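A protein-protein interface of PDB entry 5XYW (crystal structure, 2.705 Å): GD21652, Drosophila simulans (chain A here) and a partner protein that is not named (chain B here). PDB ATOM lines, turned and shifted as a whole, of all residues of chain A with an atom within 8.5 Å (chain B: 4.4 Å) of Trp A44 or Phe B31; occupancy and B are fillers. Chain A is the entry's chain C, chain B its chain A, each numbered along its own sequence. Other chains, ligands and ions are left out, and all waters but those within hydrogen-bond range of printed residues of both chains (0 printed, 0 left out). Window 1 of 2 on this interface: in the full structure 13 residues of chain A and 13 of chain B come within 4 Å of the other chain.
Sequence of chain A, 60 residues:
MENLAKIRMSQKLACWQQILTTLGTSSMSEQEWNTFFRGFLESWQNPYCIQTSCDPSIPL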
ATOM      1  N   ALA A   5      -1.391  21.035   0.643  1.00  0.00           N
ATOM      2  CA  ALA A   5      -0.501  20.663   1.735  1.00  0.00           C
ATOM      3  C   ALA A   5       0.736  21.573   1.804  1.00  0.00           C
ATOM      4  O   ALA A   5       1.431  21.774   0.807  1.00  0.00           O
ATOM      5  CB  ALA A   5      -0.083  19.199   1.595  1.00  0.00           C
ATOM      6  N   LYS A   6       1.001  22.125   2.987  1.00  0.00           N
ATOM      7  CA  LYS A   6       2.162  22.994   3.208  1.00  0.00           C
ATOM      8  C   LYS A   6       2.858  22.643   4.525  1.00  0.00           C
ATOM      9  O   LYS A   6       3.070  23.486   5.399  1.00  0.00           O
ATOM     10  CB  LYS A   6       1.746  24.463   3.188  1.00  0.00           C
ATOM     11  CG  LYS A   6       1.340  24.944   1.803  1.00  0.00           C
ATOM     12  CD  LYS A   6       1.370  26.458   1.702  1.00  0.00           C
ATOM     13  CE  LYS A   6       1.718  26.898   0.285  1.00  0.00           C
ATOM     14  NZ  LYS A   6       2.191  28.317   0.222  1.00  0.00           N
ATOM     15  N   ILE A   7       3.187  21.365   4.639  1.00  0.00           N
ATOM     16  CA  ILE A   7       3.886  20.769   5.771  1.00  0.00           C
ATOM     17  C   ILE A   7       5.331  21.232   5.873  1.00  0.00           C
ATOM     18  O   ILE A   7       5.997  21.422   4.850  1.00  0.00           O
ATOM     19  CB  ILE A   7       3.874  19.233   5.636  1.00  0.00           C
ATOM     20  CG1 ILE A   7       2.435  18.733   5.434  1.00  0.00           C
ATOM     21  CG2 ILE A   7       4.601  18.553   6.805  1.00  0.00           C
ATOM     22  CD1 ILE A   7       1.670  18.497   6.712  1.00  0.00           C
ATOM     23  N   ARG A   8       5.808  21.421   7.103  1.00  0.00           N
ATOM     24  CA  ARG A   8       7.187  21.866   7.339  1.00  0.00           C
ATOM     25  C   ARG A   8       8.188  20.713   7.361  1.00  0.00           C
ATOM     26  O   ARG A   8       7.876  19.574   7.734  1.00  0.00           O
ATOM     27  CB  ARG A   8       7.261  22.722   8.602  1.00  0.00           C
ATOM     28  CG  ARG A   8       6.692  24.104   8.285  1.00  0.00           C
ATOM     29  CD  ARG A   8       6.241  24.942   9.457  1.00  0.00           C
ATOM     30  NE  ARG A   8       5.453  26.081   8.964  1.00  0.00           N
ATOM     31  CZ  ARG A   8       4.227  25.987   8.444  1.00  0.00           C
ATOM     32  NH1 ARG A   8       3.618  24.809   8.362  1.00  0.00           N
ATOM     33  NH2 ARG A   8       3.599  27.077   8.012  1.00  0.00           N
ATOM     34  N   MET A   9       9.390  21.016   6.886  1.00  0.00           N
ATOM     35  CA  MET A   9      10.380  19.986   6.612  1.00  0.00           C
ATOM     36  C   MET A   9      10.845  19.283   7.883  1.00  0.00           C
ATOM     37  O   MET A   9      11.122  18.095   7.844  1.00  0.00           O
ATOM     38  CB  MET A   9      11.567  20.604   5.849  1.00  0.00           C
ATOM     39  CG  MET A   9      12.754  19.683   5.588  1.00  0.00           C
ATOM     40  SD  MET A   9      12.504  18.289   4.443  1.00  0.00           S
ATOM     41  CE  MET A   9      12.493  19.072   2.825  1.00  0.00           C
ATOM     42  N   GLN A  11       8.937  18.382  10.237  1.00  0.00           N
ATOM     43  CA  GLN A  11       7.919  17.353  10.416  1.00  0.00           C
ATOM     44  C   GLN A  11       8.161  16.185   9.456  1.00  0.00           C
ATOM     45  O   GLN A  11       8.062  15.015   9.851  1.00  0.00           O
ATOM     46  CB  GLN A  11       6.520  17.954  10.240  1.00  0.00           C
ATOM     47  CG  GLN A  11       6.082  18.802  11.434  1.00  0.00           C
ATOM     48  CD  GLN A  11       4.787  19.561  11.181  1.00  0.00           C
ATOM     49  OE1 GLN A  11       4.508  19.981  10.051  1.00  0.00           O
ATOM     50  NE2 GLN A  11       3.980  19.727  12.231  1.00  0.00           N
ATOM     51  N   LYS A  12       8.473  16.501   8.201  1.00  0.00           N
ATOM     52  CA  LYS A  12       8.864  15.477   7.232  1.00  0.00           C
ATOM     53  C   LYS A  12      10.069  14.648   7.727  1.00  0.00           C
ATOM     54  O   LYS A  12      10.087  13.419   7.608  1.00  0.00           O
ATOM     55  CB  LYS A  12       9.193  16.113   5.883  1.00  0.00           C
ATOM     56  CG  LYS A  12       8.042  16.850   5.206  1.00  0.00           C
ATOM     57  CD  LYS A  12       8.494  17.319   3.833  1.00  0.00           C
ATOM     58  CE  LYS A  12       7.473  18.187   3.140  1.00  0.00           C
ATOM     59  NZ  LYS A  12       7.865  18.386   1.707  1.00  0.00           N
ATOM     60  N   LEU A  13      11.095  15.325   8.241  1.00  0.00           N
ATOM     61  CA  LEU A  13      12.229  14.624   8.807  1.00  0.00           C
ATOM     62  C   LEU A  13      11.866  13.803  10.018  1.00  0.00           C
ATOM     63  O   LEU A  13      12.365  12.699  10.169  1.00  0.00           O
ATOM     64  CB  LEU A  13      13.350  15.575   9.142  1.00  0.00           C
ATOM     65  CG  LEU A  13      13.913  16.280   7.914  1.00  0.00           C
ATOM     66  CD1 LEU A  13      15.141  17.069   8.341  1.00  0.00           C
ATOM     67  CD2 LEU A  13      14.238  15.272   6.827  1.00  0.00           C
ATOM     68  N   ALA A  14      11.003  14.321  10.880  1.00  0.00           N
ATOM     69  CA  ALA A  14      10.596  13.545  12.048  1.00  0.00           C
ATOM     70  C   ALA A  14       9.919  12.243  11.578  1.00  0.00           C
ATOM     71  O   ALA A  14      10.078  11.160  12.174  1.00  0.00           O
ATOM     72  CB  ALA A  14       9.683  14.366  12.941  1.00  0.00           C
ATOM     73  N   CYS A  15       9.232  12.341  10.450  1.00  0.00           N
ATOM     74  CA  CYS A  15       8.589  11.169   9.874  1.00  0.00           C
ATOM     75  C   CYS A  15       9.607  10.190   9.311  1.00  0.00           C
ATOM     76  O   CYS A  15       9.490   8.987   9.511  1.00  0.00           O
ATOM     77  CB  CYS A  15       7.627  11.581   8.766  1.00  0.00           C
ATOM     78  SG  CYS A  15       6.141  12.288   9.431  1.00  0.00           S
ATOM     79  N   TRP A  16      10.571  10.713   8.560  1.00  0.00           N
ATOM     80  CA  TRP A  16      11.598   9.883   7.985  1.00  0.00           C
ATOM     81  C   TRP A  16      12.385   9.171   9.078  1.00  0.00           C
ATOM     82  O   TRP A  16      12.776   8.014   8.919  1.00  0.00           O
ATOM     83  CB  TRP A  16      12.526  10.697   7.115  1.00  0.00           C
ATOM     84  CG  TRP A  16      13.540   9.851   6.455  1.00  0.00           C
ATOM     85  CD1 TRP A  16      14.872   9.790   6.727  1.00  0.00           C
ATOM     86  CD2 TRP A  16      13.309   8.933   5.382  1.00  0.00           C
ATOM     87  NE1 TRP A  16      15.491   8.899   5.876  1.00  0.00           N
ATOM     88  CE2 TRP A  16      14.549   8.357   5.047  1.00  0.00           C
ATOM     89  CE3 TRP A  16      12.169   8.557   4.666  1.00  0.00           C
ATOM     90  CZ2 TRP A  16      14.682   7.417   4.036  1.00  0.00           C
ATOM     91  CZ3 TRP A  16      12.303   7.624   3.661  1.00  0.00           C
ATOM     92  CH2 TRP A  16      13.548   7.059   3.355  1.00  0.00           C
ATOM     93  N   GLN A  17      12.606   9.863  10.191  1.00  0.00           N
ATOM     94  CA  GLN A  17      13.359   9.287  11.285  1.00  0.00           C
ATOM     95  C   GLN A  17      12.546   8.158  11.918  1.00  0.00           C
ATOM     96  O   GLN A  17      13.094   7.091  12.244  1.00  0.00           O
ATOM     97  CB  GLN A  17      13.712  10.369  12.314  1.00  0.00           C
ATOM     98  CG  GLN A  17      14.707  11.410  11.762  1.00  0.00           C
ATOM     99  CD  GLN A  17      15.046  12.548  12.732  1.00  0.00           C
ATOM    100  OE1 GLN A  17      14.302  13.529  12.855  1.00  0.00           O
ATOM    101  NE2 GLN A  17      16.212  12.453  13.366  1.00  0.00           N
ATOM    102  N   GLN A  18      11.229   8.366  12.015  1.00  0.00           N
ATOM    103  CA  GLN A  18      10.318   7.310  12.477  1.00  0.00           C
ATOM    104  C   GLN A  18      10.304   6.115  11.513  1.00  0.00           C
ATOM    105  O   GLN A  18      10.221   4.960  11.934  1.00  0.00           O
ATOM    106  CB  GLN A  18       8.897   7.875  12.680  1.00  0.00           C
ATOM    107  CG  GLN A  18       8.753   8.664  13.979  1.00  0.00           C
ATOM    108  CD  GLN A  18       7.596   9.667  13.997  1.00  0.00           C
ATOM    109  OE1 GLN A  18       6.932   9.918  12.986  1.00  0.00           O
ATOM    110  NE2 GLN A  18       7.321  10.209  15.179  1.00  0.00           N
ATOM    111  N   ILE A  19      10.461   6.390  10.227  1.00  0.00           N
ATOM    112  CA  ILE A  19      10.511   5.343   9.224  1.00  0.00           C
ATOM    113  C   ILE A  19      11.784   4.497   9.417  1.00  0.00           C
ATOM    114  O   ILE A  19      11.727   3.257   9.468  1.00  0.00           O
ATOM    115  CB  ILE A  19      10.420   5.958   7.788  1.00  0.00           C
ATOM    116  CG1 ILE A  19       8.962   6.349   7.486  1.00  0.00           C
ATOM    117  CG2 ILE A  19      10.863   4.979   6.710  1.00  0.00           C
ATOM    118  CD1 ILE A  19       8.739   7.032   6.107  1.00  0.00           C
ATOM    119  N   PHE A  37      14.328   7.707  -0.118  1.00  0.00           N
ATOM    120  CA  PHE A  37      14.250   9.020   0.502  1.00  0.00           C
ATOM    121  C   PHE A  37      13.906  10.103  -0.517  1.00  0.00           C
ATOM    122  O   PHE A  37      13.171  11.051  -0.222  1.00  0.00           O
ATOM    123  CB  PHE A  37      15.560   9.372   1.191  1.00  0.00           C
ATOM    124  CG  PHE A  37      15.540  10.696   1.871  1.00  0.00           C
ATOM    125  CD1 PHE A  37      14.777  10.875   3.008  1.00  0.00           C
ATOM    126  CD2 PHE A  37      16.244  11.772   1.372  1.00  0.00           C
ATOM    127  CE1 PHE A  37      14.729  12.098   3.658  1.00  0.00           C
ATOM    128  CE2 PHE A  37      16.197  13.001   2.014  1.00  0.00           C
ATOM    129  CZ  PHE A  37      15.436  13.159   3.161  1.00  0.00           C
ATOM    130  N   ARG A  38      14.414   9.956  -1.727  1.00  0.00           N
ATOM    131  CA  ARG A  38      14.136  10.942  -2.752  1.00  0.00           C
ATOM    132  C   ARG A  38      12.654  10.769  -3.134  1.00  0.00           C
ATOM    133  O   ARG A  38      11.912  11.756  -3.345  1.00  0.00           O
ATOM    134  CB  ARG A  38      15.100  10.755  -3.948  1.00  0.00           C
ATOM    135  CG  ARG A  38      15.007  11.838  -5.040  1.00  0.00           C
ATOM    136  CD  ARG A  38      15.757  11.558  -6.354  1.00  0.00           C
ATOM    137  NE  ARG A  38      15.383  12.547  -7.381  1.00  0.00           N
ATOM    138  CZ  ARG A  38      14.352  12.432  -8.222  1.00  0.00           C
ATOM    139  NH1 ARG A  38      13.576  11.354  -8.174  1.00  0.00           N
ATOM    140  NH2 ARG A  38      14.092  13.396  -9.108  1.00  0.00           N
ATOM    141  N   GLY A  39      12.189   9.518  -3.135  1.00  0.00           N
ATOM    142  CA  GLY A  39      10.774   9.275  -3.394  1.00  0.00           C
ATOM    143  C   GLY A  39       9.845   9.794  -2.288  1.00  0.00           C
ATOM    144  O   GLY A  39       8.758  10.304  -2.538  1.00  0.00           O
ATOM    145  N   PHE A  40      10.317   9.698  -1.057  1.00  0.00           N
ATOM    146  CA  PHE A  40       9.622  10.198   0.094  1.00  0.00           C
ATOM    147  C   PHE A  40       9.459  11.691   0.012  1.00  0.00           C
ATOM    148  O   PHE A  40       8.453  12.230   0.458  1.00  0.00           O
ATOM    149  CB  PHE A  40      10.353   9.806   1.367  1.00  0.00           C
ATOM    150  CG  PHE A  40       9.828  10.498   2.606  1.00  0.00           C
ATOM    151  CD1 PHE A  40       8.678  10.041   3.242  1.00  0.00           C
ATOM    152  CD2 PHE A  40      10.517  11.590   3.153  1.00  0.00           C
ATOM    153  CE1 PHE A  40       8.205  10.670   4.387  1.00  0.00           C
ATOM    154  CE2 PHE A  40      10.061  12.207   4.295  1.00  0.00           C
ATOM    155  CZ  PHE A  40       8.892  11.750   4.913  1.00  0.00           C
ATOM    156  N   LEU A  41      10.467  12.375  -0.507  1.00  0.00           N
ATOM    157  CA  LEU A  41      10.347  13.826  -0.636  1.00  0.00           C
ATOM    158  C   LEU A  41       9.394  14.220  -1.753  1.00  0.00           C
ATOM    159  O   LEU A  41       8.513  15.065  -1.553  1.00  0.00           O
ATOM    160  CB  LEU A  41      11.706  14.457  -0.867  1.00  0.00           C
ATOM    161  CG  LEU A  41      12.547  14.326   0.395  1.00  0.00           C
ATOM    162  CD1 LEU A  41      13.972  14.767   0.150  1.00  0.00           C
ATOM    163  CD2 LEU A  41      11.921  15.134   1.518  1.00  0.00           C
ATOM    164  N   GLU A  42       9.539  13.608  -2.923  1.00  0.00           N
ATOM    165  CA  GLU A  42       8.657  13.986  -4.025  1.00  0.00           C
ATOM    166  C   GLU A  42       7.210  13.548  -3.735  1.00  0.00           C
ATOM    167  O   GLU A  42       6.254  13.995  -4.371  1.00  0.00           O
ATOM    168  CB  GLU A  42       9.163  13.367  -5.322  1.00  0.00           C
ATOM    169  CG  GLU A  42      10.542  13.835  -5.707  1.00  0.00           C
ATOM    170  CD  GLU A  42      11.118  13.102  -6.905  1.00  0.00           C
ATOM    171  OE1 GLU A  42      11.740  13.776  -7.756  1.00  0.00           O
ATOM    172  OE2 GLU A  42      10.960  11.861  -6.995  1.00  0.00           O
ATOM    173  N   SER A  43       7.072  12.671  -2.749  1.00  0.00           N
ATOM    174  CA  SER A  43       5.788  12.224  -2.238  1.00  0.00           C
ATOM    175  C   SER A  43       4.856  13.337  -1.754  1.00  0.00           C
ATOM    176  O   SER A  43       3.702  13.400  -2.151  1.00  0.00           O
ATOM    177  CB  SER A  43       6.048  11.251  -1.097  1.00  0.00           C
ATOM    178  OG  SER A  43       4.908  11.094  -0.294  1.00  0.00           O
ATOM    179  N   TRP A  44       5.367  14.221  -0.907  1.00  0.00           N
ATOM    180  CA  TRP A  44       4.592  15.354  -0.416  1.00  0.00           C
ATOM    181  C   TRP A  44       4.247  16.309  -1.554  1.00  0.00           C
ATOM    182  O   TRP A  44       3.302  17.092  -1.458  1.00  0.00           O
ATOM    183  CB  TRP A  44       5.363  16.070   0.701  1.00  0.00           C
ATOM    184  CG  TRP A  44       5.774  15.097   1.738  1.00  0.00           C
ATOM    185  CD1 TRP A  44       6.881  14.300   1.707  1.00  0.00           C
ATOM    186  CD2 TRP A  44       5.059  14.747   2.924  1.00  0.00           C
ATOM    187  NE1 TRP A  44       6.916  13.492   2.811  1.00  0.00           N
ATOM    188  CE2 TRP A  44       5.805  13.741   3.577  1.00  0.00           C
ATOM    189  CE3 TRP A  44       3.869  15.185   3.510  1.00  0.00           C
ATOM    190  CZ2 TRP A  44       5.392  13.166   4.786  1.00  0.00           C
ATOM    191  CZ3 TRP A  44       3.469  14.616   4.720  1.00  0.00           C
ATOM    192  CH2 TRP A  44       4.228  13.613   5.335  1.00  0.00           C
ATOM    193  N   GLN A  45       5.012  16.238  -2.638  1.00  0.00           N
ATOM    194  CA  GLN A  45       4.823  17.150  -3.762  1.00  0.00           C
ATOM    195  C   GLN A  45       3.657  16.712  -4.647  1.00  0.00           C
ATOM    196  O   GLN A  45       3.675  16.915  -5.864  1.00  0.00           O
ATOM    197  CB  GLN A  45       6.104  17.253  -4.581  1.00  0.00           C
ATOM    198  N   VAL B  19      -5.682  11.189   8.755  1.00  0.00           N
ATOM    199  CA  VAL B  19      -4.688  10.525   7.937  1.00  0.00           C
ATOM    200  C   VAL B  19      -4.310  11.510   6.872  1.00  0.00           C
ATOM    201  O   VAL B  19      -5.070  11.739   5.944  1.00  0.00           O
ATOM    202  CB  VAL B  19      -5.195   9.243   7.271  1.00  0.00           C
ATOM    203  CG1 VAL B  19      -4.072   8.628   6.440  1.00  0.00           C
ATOM    204  CG2 VAL B  19      -5.697   8.269   8.304  1.00  0.00           C
ATOM    205  N   LEU B  20      -3.133  12.099   7.014  1.00  0.00           N
ATOM    206  CA  LEU B  20      -2.703  13.174   6.131  1.00  0.00           C
ATOM    207  C   LEU B  20      -2.166  12.684   4.802  1.00  0.00           C
ATOM    208  O   LEU B  20      -2.449  13.279   3.763  1.00  0.00           O
ATOM    209  CB  LEU B  20      -1.641  14.029   6.822  1.00  0.00           C
ATOM    210  CG  LEU B  20      -2.124  14.660   8.129  1.00  0.00           C
ATOM    211  CD1 LEU B  20      -1.134  15.704   8.640  1.00  0.00           C
ATOM    212  CD2 LEU B  20      -3.513  15.264   7.939  1.00  0.00           C
ATOM    213  N   HIS B  21      -1.392  11.608   4.817  1.00  0.00           N
ATOM    214  CA  HIS B  21      -0.644  11.282   3.599  1.00  0.00           C
ATOM    215  C   HIS B  21      -0.188   9.841   3.671  1.00  0.00           C
ATOM    216  O   HIS B  21      -0.314   9.211   4.709  1.00  0.00           O
ATOM    217  CB  HIS B  21       0.530  12.278   3.453  1.00  0.00           C
ATOM    218  CG  HIS B  21       1.468  12.011   2.310  1.00  0.00           C
ATOM    219  ND1 HIS B  21       1.038  11.724   1.029  1.00  0.00           N
ATOM    220  CD2 HIS B  21       2.821  12.031   2.254  1.00  0.00           C
ATOM    221  CE1 HIS B  21       2.086  11.556   0.242  1.00  0.00           C
ATOM    222  NE2 HIS B  21       3.181  11.736   0.962  1.00  0.00           N
ATOM    223  N   CYS B  22       0.319   9.290   2.578  1.00  0.00           N
ATOM    224  CA  CYS B  22       0.899   7.958   2.675  1.00  0.00           C
ATOM    225  C   CYS B  22       2.153   7.812   1.811  1.00  0.00           C
ATOM    226  O   CYS B  22       2.377   8.600   0.890  1.00  0.00           O
ATOM    227  CB  CYS B  22      -0.146   6.905   2.285  1.00  0.00           C
ATOM    228  SG  CYS B  22      -0.232   6.652   0.504  1.00  0.00           S
ATOM    229  N   TYR B  23       2.979   6.809   2.119  1.00  0.00           N
ATOM    230  CA  TYR B  23       4.151   6.496   1.288  1.00  0.00           C
ATOM    231  C   TYR B  23       4.470   4.999   1.326  1.00  0.00           C
ATOM    232  O   TYR B  23       4.645   4.382   2.377  1.00  0.00           O
ATOM    233  CB  TYR B  23       5.378   7.325   1.714  1.00  0.00           C
ATOM    234  CG  TYR B  23       6.540   7.168   0.764  1.00  0.00           C
ATOM    235  CD1 TYR B  23       6.484   7.695  -0.523  1.00  0.00           C
ATOM    236  CD2 TYR B  23       7.685   6.452   1.130  1.00  0.00           C
ATOM    237  CE1 TYR B  23       7.542   7.518  -1.429  1.00  0.00           C
ATOM    238  CE2 TYR B  23       8.750   6.290   0.246  1.00  0.00           C
ATOM    239  CZ  TYR B  23       8.665   6.815  -1.031  1.00  0.00           C
ATOM    240  OH  TYR B  23       9.721   6.635  -1.891  1.00  0.00           O
ATOM    241  N   PHE B  29       3.323   3.259   4.647  1.00  0.00           N
ATOM    242  CA  PHE B  29       3.303   4.139   5.802  1.00  0.00           C
ATOM    243  C   PHE B  29       2.204   5.156   5.665  1.00  0.00           C
ATOM    244  O   PHE B  29       1.980   5.689   4.584  1.00  0.00           O
ATOM    245  CB  PHE B  29       4.642   4.857   5.979  1.00  0.00           C
ATOM    246  CG  PHE B  29       5.634   4.068   6.750  1.00  0.00           C
ATOM    247  CD1 PHE B  29       5.549   4.004   8.132  1.00  0.00           C
ATOM    248  CD2 PHE B  29       6.628   3.360   6.094  1.00  0.00           C
ATOM    249  CE1 PHE B  29       6.454   3.252   8.849  1.00  0.00           C
ATOM    250  CE2 PHE B  29       7.524   2.599   6.796  1.00  0.00           C
ATOM    251  CZ  PHE B  29       7.457   2.546   8.173  1.00  0.00           C
ATOM    252  N   LEU B  30       1.515   5.409   6.764  1.00  0.00           N
ATOM    253  CA  LEU B  30       0.528   6.459   6.797  1.00  0.00           C
ATOM    254  C   LEU B  30       1.060   7.524   7.696  1.00  0.00           C
ATOM    255  O   LEU B  30       1.575   7.246   8.775  1.00  0.00           O
ATOM    256  CB  LEU B  30      -0.844   5.972   7.298  1.00  0.00           C
ATOM    257  CG  LEU B  30      -1.526   4.793   6.595  1.00  0.00           C
ATOM    258  CD1 LEU B  30      -2.972   4.798   6.962  1.00  0.00           C
ATOM    259  CD2 LEU B  30      -1.355   4.816   5.077  1.00  0.00           C
ATOM    260  N   PHE B  31       0.927   8.748   7.225  1.00  0.00           N
ATOM    261  CA  PHE B  31       1.303   9.906   7.982  1.00  0.00           C
ATOM    262  C   PHE B  31       0.048  10.539   8.554  1.00  0.00           C
ATOM    263  O   PHE B  31      -0.775  11.136   7.825  1.00  0.00           O
ATOM    264  CB  PHE B  31       2.104  10.836   7.086  1.00  0.00           C
ATOM    265  CG  PHE B  31       3.243  10.133   6.415  1.00  0.00           C
ATOM    266  CD1 PHE B  31       4.400   9.813   7.137  1.00  0.00           C
ATOM    267  CD2 PHE B  31       3.143   9.722   5.094  1.00  0.00           C
ATOM    268  CE1 PHE B  31       5.455   9.133   6.541  1.00  0.00           C
ATOM    269  CE2 PHE B  31       4.205   9.042   4.486  1.00  0.00           C
ATOM    270  CZ  PHE B  31       5.365   8.747   5.218  1.00  0.00           C
ATOM    271  N   VAL B  32      -0.083  10.344   9.866  1.00  0.00           N
ATOM    272  CA  VAL B  32      -1.272  10.672  10.623  1.00  0.00           C
ATOM    273  C   VAL B  32      -1.021  11.660  11.755  1.00  0.00           C
ATOM    274  O   VAL B  32       0.057  11.691  12.346  1.00  0.00           O
ATOM    275  CB  VAL B  32      -1.893   9.413  11.259  1.00  0.00           C
ATOM    276  CG1 VAL B  32      -2.220   8.363  10.209  1.00  0.00           C
ATOM    277  CG2 VAL B  32      -0.974   8.855  12.316  1.00  0.00           C
ATOM    278  N   ILE B  40       2.899  15.016  13.394  1.00  0.00           N
ATOM    279  CA  ILE B  40       2.596  13.973  12.426  1.00  0.00           C
ATOM    280  C   ILE B  40       3.499  12.782  12.675  1.00  0.00           C
ATOM    281  O   ILE B  40       4.673  12.940  13.006  1.00  0.00           O
ATOM    282  CB  ILE B  40       2.795  14.469  10.990  1.00  0.00           C
ATOM    283  CG1 ILE B  40       2.167  15.858  10.843  1.00  0.00           C
ATOM    284  CG2 ILE B  40       2.261  13.465   9.986  1.00  0.00           C
ATOM    285  CD1 ILE B  40       2.497  16.549   9.559  1.00  0.00           C
ATOM    286  N   ASP B  41       2.940  11.593  12.540  1.00  0.00           N
ATOM    287  CA  ASP B  41       3.672  10.372  12.783  1.00  0.00           C
ATOM    288  C   ASP B  41       3.565   9.487  11.569  1.00  0.00           C
ATOM    289  O   ASP B  41       2.521   9.447  10.899  1.00  0.00           O
ATOM    290  CB  ASP B  41       3.150   9.634  14.014  1.00  0.00           C
ATOM    291  CG  ASP B  41       3.513  10.326  15.293  1.00  0.00           C
ATOM    292  OD1 ASP B  41       3.972  11.485  15.230  1.00  0.00           O
ATOM    293  OD2 ASP B  41       3.333   9.718  16.364  1.00  0.00           O
ATOM    294  N   ALA B  42       4.673   8.810  11.275  1.00  0.00           N
ATOM    295  CA  ALA B  42       4.681   7.746  10.298  1.00  0.00           C
ATOM    296  C   ALA B  42       4.272   6.507  11.060  1.00  0.00           C
ATOM    297  O   ALA B  42       4.831   6.214  12.119  1.00  0.00           O
ATOM    298  CB  ALA B  42       6.039   7.590   9.673  1.00  0.00           C
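OH of Tyr B23 sits at hydrogen-bond distance from N of Phe A40, 3.2 Å away.
N of Ala B42 is in hydrogen-bond range of OE1 of Gln A18.
The side-chain hydroxyl of Ser A43 sits close to a ring nitrogen (NE2) of His B21 (2.2 Å).
Printed residues of chain B within 4 Å of Gln A18: Ile B40 (3.8 Å), Asp B41 (3.3 Å) and Ala B42 (3.0 Å).
Printed residues of chain B within 4 Å of Ile A19: Phe B31 and Ala B42.
Of the printed residues of chain B, Phe A40 touches Tyr B23 and Phe B31.
Printed residues of chain B within 4 Å of Trp A44: His B21 (3.6 Å) and Phe B31 (3.8 Å).
Val B19 touches none of the printed residues of chain A.
Phe B31 touches just these residues of chain A: Cys A15 (3.8 Å), Ile A19 (3.9 Å), Phe A40 (3.5 Å) and Trp A44 (3.8 Å).
The nearest printed residue of chain B that does not touch Trp A44 is Ile B40 (5.1 Å).
The nearest residue of chain A that does not touch Phe B31 is Ser A43 (5.2 Å).
N of Leu B20 sits at hydrogen-bond distance from O of Phe B31, at 2.7 Å.
The backbone carbonyl oxygen of His B21 lies within hydrogen-bond range of the backbone NH of Phe B31 (2.8 Å).
The backbone carbonyl oxygen of Tyr B23 sits at hydrogen-bond distance from the backbone NH of Phe B29, 2.9 Å away.
The backbone carbonyl oxygen (O) of Val B32 lies within hydrogen-bond range of the backbone NH (N) of Asp B41 (2.9 Å).
O of Ala A14 lies close to OE1 of Gln A18, at 3.5 Å.
O of Phe A40 lies close to NE1 of Trp A44.
Among the printed residues, merely in contact across the chains: Gly A39 with Tyr B23 (3.2 Å), Gln A18 with Asp B41 (3.3 Å), Phe A40 with Phe B31 (3.5 Å), Ile A7 with Ile B40 (3.5 Å), Trp A44 with His B21 (3.6 Å), Ser A43 with Tyr B23 (3.6 Å), Cys A15 with Ala B42 (3.7 Å), Ser A43 with Cys B22 (3.7 Å), Gln A18 with Ile B40 (3.8 Å), Trp A44 with Phe B31 (3.8 Å), Cys A15 with Phe B31 (3.8 Å), Ile A19 with Ala B42 (3.9 Å), Ile A19 with Phe B31 (3.9 Å) and Cys A15 with Ile B40 (3.9 Å).
Of the 23 printed residues of chain A, 8 touch a printed residue of chain B.
Along chain A the printed residues that touch a printed residue of chain B span positions 7 to 44.
Among the printed residues, 17 pairs touch across the chains.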
